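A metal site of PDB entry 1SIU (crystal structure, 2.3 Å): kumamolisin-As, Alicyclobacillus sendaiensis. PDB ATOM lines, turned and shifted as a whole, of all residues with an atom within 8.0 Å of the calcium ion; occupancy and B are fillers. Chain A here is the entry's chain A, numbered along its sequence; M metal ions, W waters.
The side-chain carboxylate (OD1) of Asp 338 is in hydrogen-bond range of the side-chain hydroxyl (OG1) of Thr 341.
OD1 of Asp 338 lies close to N of Cys 340 (3.2 Å).
The calcium ion is bound by O of Gly 334 (2.3 Å), OD1 of Asp 316 (2.3 Å), O of Ile 317 (2.3 Å), O of Gly 336 (2.3 Å), water W1 (2.3 Å) and OD2 of Asp 338 (2.3 Å).
Merely in contact with the calcium ion: Pro 335.
Of the 20 residues printed, 6 come within 4 Å of the calcium ion.
Water W1 lies within hydrogen-bond range of the backbone carbonyl oxygen of Gly 342 (2.7 Å), the side-chain hydroxyl of Thr 341 (2.9 Å), the backbone NH of Ile 317 (3.3 Å) and the backbone NH of Gly 344 (3.5 Å).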
ATOM      1  N   VAL A 207      -9.789  -9.821   5.276  1.00  0.00           N
ATOM      2  CA  VAL A 207      -9.670 -11.261   5.403  1.00  0.00           C
ATOM      3  C   VAL A 207     -10.537 -11.962   4.365  1.00  0.00           C
ATOM      4  O   VAL A 207     -11.679 -11.574   4.070  1.00  0.00           O
ATOM      5  CB  VAL A 207     -10.089 -11.803   6.794  1.00  0.00           C
ATOM      6  CG1 VAL A 207      -9.963 -13.315   6.755  1.00  0.00           C
ATOM      7  CG2 VAL A 207      -9.284 -11.215   7.931  1.00  0.00           C
ATOM      8  N   HIS A 315       1.658  -4.250   5.010  1.00  0.00           N
ATOM      9  CA  HIS A 315       0.325  -3.673   4.919  1.00  0.00           C
ATOM     10  C   HIS A 315      -0.588  -4.467   5.852  1.00  0.00           C
ATOM     11  O   HIS A 315      -1.071  -5.579   5.645  1.00  0.00           O
ATOM     12  CB  HIS A 315      -0.196  -3.683   3.488  1.00  0.00           C
ATOM     13  CG  HIS A 315      -1.545  -3.025   3.473  1.00  0.00           C
ATOM     14  ND1 HIS A 315      -2.719  -3.732   3.605  1.00  0.00           N
ATOM     15  CD2 HIS A 315      -1.887  -1.718   3.366  1.00  0.00           C
ATOM     16  CE1 HIS A 315      -3.727  -2.883   3.561  1.00  0.00           C
ATOM     17  NE2 HIS A 315      -3.257  -1.654   3.420  1.00  0.00           N
ATOM     18  N   ASP A 316      -0.850  -3.868   7.010  1.00  0.00           N
ATOM     19  CA  ASP A 316      -1.600  -4.561   8.054  1.00  0.00           C
ATOM     20  C   ASP A 316      -3.053  -4.839   7.740  1.00  0.00           C
ATOM     21  O   ASP A 316      -3.811  -3.917   7.407  1.00  0.00           O
ATOM     22  CB  ASP A 316      -1.536  -3.708   9.331  1.00  0.00           C
ATOM     23  CG  ASP A 316      -2.218  -4.435  10.466  1.00  0.00           C
ATOM     24  OD1 ASP A 316      -2.374  -5.650  10.331  1.00  0.00           O
ATOM     25  OD2 ASP A 316      -2.566  -3.771  11.463  1.00  0.00           O
ATOM     26  N   ILE A 317      -3.521  -6.091   7.852  1.00  0.00           N
ATOM     27  CA  ILE A 317      -4.963  -6.251   7.613  1.00  0.00           C
ATOM     28  C   ILE A 317      -5.706  -6.342   8.931  1.00  0.00           C
ATOM     29  O   ILE A 317      -5.380  -7.196   9.754  1.00  0.00           O
ATOM     30  CB  ILE A 317      -5.236  -7.480   6.744  1.00  0.00           C
ATOM     31  CG1 ILE A 317      -4.973  -7.230   5.256  1.00  0.00           C
ATOM     32  CG2 ILE A 317      -6.654  -7.979   6.962  1.00  0.00           C
ATOM     33  CD1 ILE A 317      -3.661  -7.780   4.754  1.00  0.00           C
ATOM     34  N   THR A 318      -6.662  -5.444   9.096  1.00  0.00           N
ATOM     35  CA  THR A 318      -7.422  -5.271  10.319  1.00  0.00           C
ATOM     36  C   THR A 318      -8.917  -5.575  10.256  1.00  0.00           C
ATOM     37  O   THR A 318      -9.537  -5.437  11.308  1.00  0.00           O
ATOM     38  CB  THR A 318      -7.393  -3.798  10.825  1.00  0.00           C
ATOM     39  OG1 THR A 318      -8.044  -2.950   9.856  1.00  0.00           O
ATOM     40  CG2 THR A 318      -5.965  -3.336  11.004  1.00  0.00           C
ATOM     41  N   GLU A 319      -9.524  -5.958   9.157  1.00  0.00           N
ATOM     42  CA  GLU A 319     -10.965  -6.222   9.121  1.00  0.00           C
ATOM     43  C   GLU A 319     -11.269  -7.626   8.635  1.00  0.00           C
ATOM     44  O   GLU A 319     -10.546  -8.105   7.745  1.00  0.00           O
ATOM     45  CB  GLU A 319     -11.585  -5.178   8.199  1.00  0.00           C
ATOM     46  CG  GLU A 319     -12.960  -5.512   7.649  1.00  0.00           C
ATOM     47  CD  GLU A 319     -13.669  -4.222   7.229  1.00  0.00           C
ATOM     48  OE1 GLU A 319     -13.120  -3.156   7.587  1.00  0.00           O
ATOM     49  OE2 GLU A 319     -14.725  -4.300   6.568  1.00  0.00           O
ATOM     50  N   GLN A 332     -10.402 -13.660  14.339  1.00  0.00           N
ATOM     51  CA  GLN A 332     -10.629 -12.341  13.759  1.00  0.00           C
ATOM     52  C   GLN A 332      -9.364 -11.542  13.489  1.00  0.00           C
ATOM     53  O   GLN A 332      -8.320 -11.721  14.134  1.00  0.00           O
ATOM     54  CB  GLN A 332     -11.513 -11.529  14.712  1.00  0.00           C
ATOM     55  CG  GLN A 332     -12.656 -10.820  13.993  1.00  0.00           C
ATOM     56  CD  GLN A 332     -12.990  -9.576  14.802  1.00  0.00           C
ATOM     57  OE1 GLN A 332     -13.206  -8.519  14.199  1.00  0.00           O
ATOM     58  NE2 GLN A 332     -13.008  -9.762  16.118  1.00  0.00           N
ATOM     59  N   ALA A 333      -9.482 -10.646  12.504  1.00  0.00           N
ATOM     60  CA  ALA A 333      -8.341  -9.840  12.115  1.00  0.00           C
ATOM     61  C   ALA A 333      -8.178  -8.691  13.083  1.00  0.00           C
ATOM     62  O   ALA A 333      -9.130  -8.405  13.811  1.00  0.00           O
ATOM     63  CB  ALA A 333      -8.543  -9.426  10.666  1.00  0.00           C
ATOM     64  N   GLY A 334      -7.020  -8.019  13.137  1.00  0.00           N
ATOM     65  CA  GLY A 334      -6.926  -6.917  14.093  1.00  0.00           C
ATOM     66  C   GLY A 334      -5.606  -6.190  13.889  1.00  0.00           C
ATOM     67  O   GLY A 334      -4.904  -6.440  12.910  1.00  0.00           O
ATOM     68  N   PRO A 335      -5.218  -5.285  14.779  1.00  0.00           N
ATOM     69  CA  PRO A 335      -3.928  -4.615  14.624  1.00  0.00           C
ATOM     70  C   PRO A 335      -2.749  -5.585  14.711  1.00  0.00           C
ATOM     71  O   PRO A 335      -2.813  -6.515  15.527  1.00  0.00           O
ATOM     72  CB  PRO A 335      -3.883  -3.653  15.823  1.00  0.00           C
ATOM     73  CG  PRO A 335      -5.305  -3.496  16.265  1.00  0.00           C
ATOM     74  CD  PRO A 335      -5.966  -4.815  15.959  1.00  0.00           C
ATOM     75  N   GLY A 336      -1.723  -5.338  13.896  1.00  0.00           N
ATOM     76  CA  GLY A 336      -0.510  -6.158  13.837  1.00  0.00           C
ATOM     77  C   GLY A 336      -0.872  -7.602  13.495  1.00  0.00           C
ATOM     78  O   GLY A 336      -1.869  -7.772  12.759  1.00  0.00           O
ATOM     79  N   TRP A 337      -0.108  -8.542  14.018  1.00  0.00           N
ATOM     80  CA  TRP A 337      -0.305  -9.975  13.836  1.00  0.00           C
ATOM     81  C   TRP A 337      -1.689 -10.410  14.306  1.00  0.00           C
ATOM     82  O   TRP A 337      -2.097 -10.064  15.409  1.00  0.00           O
ATOM     83  CB  TRP A 337       0.719 -10.860  14.591  1.00  0.00           C
ATOM     84  CG  TRP A 337       0.644 -12.267  14.038  1.00  0.00           C
ATOM     85  CD1 TRP A 337       1.339 -12.791  12.985  1.00  0.00           C
ATOM     86  CD2 TRP A 337      -0.193 -13.326  14.524  1.00  0.00           C
ATOM     87  NE1 TRP A 337       0.998 -14.113  12.789  1.00  0.00           N
ATOM     88  CE2 TRP A 337       0.053 -14.455  13.718  1.00  0.00           C
ATOM     89  CE3 TRP A 337      -1.112 -13.405  15.567  1.00  0.00           C
ATOM     90  CZ2 TRP A 337      -0.595 -15.671  13.929  1.00  0.00           C
ATOM     91  CZ3 TRP A 337      -1.758 -14.608  15.760  1.00  0.00           C
ATOM     92  CH2 TRP A 337      -1.507 -15.730  14.948  1.00  0.00           C
ATOM     93  N   ASP A 338      -2.362 -11.161  13.449  1.00  0.00           N
ATOM     94  CA  ASP A 338      -3.652 -11.797  13.726  1.00  0.00           C
ATOM     95  C   ASP A 338      -3.676 -13.204  13.124  1.00  0.00           C
ATOM     96  O   ASP A 338      -2.953 -13.529  12.176  1.00  0.00           O
ATOM     97  CB  ASP A 338      -4.797 -10.921  13.255  1.00  0.00           C
ATOM     98  CG  ASP A 338      -4.978 -10.562  11.806  1.00  0.00           C
ATOM     99  OD1 ASP A 338      -5.267 -11.459  10.958  1.00  0.00           O
ATOM    100  OD2 ASP A 338      -4.830  -9.356  11.462  1.00  0.00           O
ATOM    101  N   PRO A 339      -4.498 -14.104  13.649  1.00  0.00           N
ATOM    102  CA  PRO A 339      -4.544 -15.484  13.177  1.00  0.00           C
ATOM    103  C   PRO A 339      -5.441 -15.706  11.963  1.00  0.00           C
ATOM    104  O   PRO A 339      -5.921 -16.819  11.739  1.00  0.00           O
ATOM    105  CB  PRO A 339      -5.098 -16.255  14.404  1.00  0.00           C
ATOM    106  CG  PRO A 339      -5.256 -15.235  15.484  1.00  0.00           C
ATOM    107  CD  PRO A 339      -5.451 -13.913  14.764  1.00  0.00           C
ATOM    108  N   CYS A 340      -5.629 -14.648  11.195  1.00  0.00           N
ATOM    109  CA  CYS A 340      -6.268 -14.673   9.906  1.00  0.00           C
ATOM    110  C   CYS A 340      -5.284 -14.324   8.773  1.00  0.00           C
ATOM    111  O   CYS A 340      -5.274 -14.934   7.719  1.00  0.00           O
ATOM    112  CB  CYS A 340      -7.411 -13.653   9.765  1.00  0.00           C
ATOM    113  SG  CYS A 340      -8.788 -13.885  10.900  1.00  0.00           S
ATOM    114  N   THR A 341      -4.461 -13.303   8.985  1.00  0.00           N
ATOM    115  CA  THR A 341      -3.616 -12.783   7.924  1.00  0.00           C
ATOM    116  C   THR A 341      -2.176 -12.633   8.376  1.00  0.00           C
ATOM    117  O   THR A 341      -1.266 -12.197   7.678  1.00  0.00           O
ATOM    118  CB  THR A 341      -4.136 -11.413   7.439  1.00  0.00           C
ATOM    119  OG1 THR A 341      -4.289 -10.580   8.592  1.00  0.00           O
ATOM    120  CG2 THR A 341      -5.490 -11.498   6.731  1.00  0.00           C
ATOM    121  N   GLY A 342      -1.906 -13.010   9.630  1.00  0.00           N
ATOM    122  CA  GLY A 342      -0.529 -12.838  10.057  1.00  0.00           C
ATOM    123  C   GLY A 342      -0.120 -11.380  10.173  1.00  0.00           C
ATOM    124  O   GLY A 342      -0.904 -10.557  10.639  1.00  0.00           O
ATOM    125  N   LEU A 343       1.114 -11.122   9.768  1.00  0.00           N
ATOM    126  CA  LEU A 343       1.697  -9.807   9.788  1.00  0.00           C
ATOM    127  C   LEU A 343       0.983  -8.894   8.775  1.00  0.00           C
ATOM    128  O   LEU A 343       1.107  -7.691   8.998  1.00  0.00           O
ATOM    129  CB  LEU A 343       3.192  -9.798   9.467  1.00  0.00           C
ATOM    130  CG  LEU A 343       4.140 -10.478  10.452  1.00  0.00           C
ATOM    131  CD1 LEU A 343       5.546 -10.537   9.863  1.00  0.00           C
ATOM    132  CD2 LEU A 343       4.148  -9.747  11.781  1.00  0.00           C
ATOM    133  N   GLY A 344       0.346  -9.486   7.784  1.00  0.00           N
ATOM    134  CA  GLY A 344      -0.419  -8.920   6.691  1.00  0.00           C
ATOM    135  C   GLY A 344       0.208  -9.116   5.319  1.00  0.00           C
ATOM    136  O   GLY A 344       1.005 -10.034   5.100  1.00  0.00           O
ATOM    137  N   SER A 345      -0.106  -8.276   4.333  1.00  0.00           N
ATOM    138  CA  SER A 345       0.543  -8.354   3.026  1.00  0.00           C
ATOM    139  C   SER A 345       1.894  -7.660   2.976  1.00  0.00           C
ATOM    140  O   SER A 345       2.018  -6.490   3.383  1.00  0.00           O
ATOM    141  CB  SER A 345      -0.328  -7.696   1.927  1.00  0.00           C
ATOM    142  OG  SER A 345      -0.274  -6.291   2.153  1.00  0.00           O
HETATM  143 CA    CA M   1      -3.610  -7.373  11.259  1.00  0.00          CA
HETATM  144  O   HOH W   1      -2.407  -8.592   9.670  1.00  0.00           O
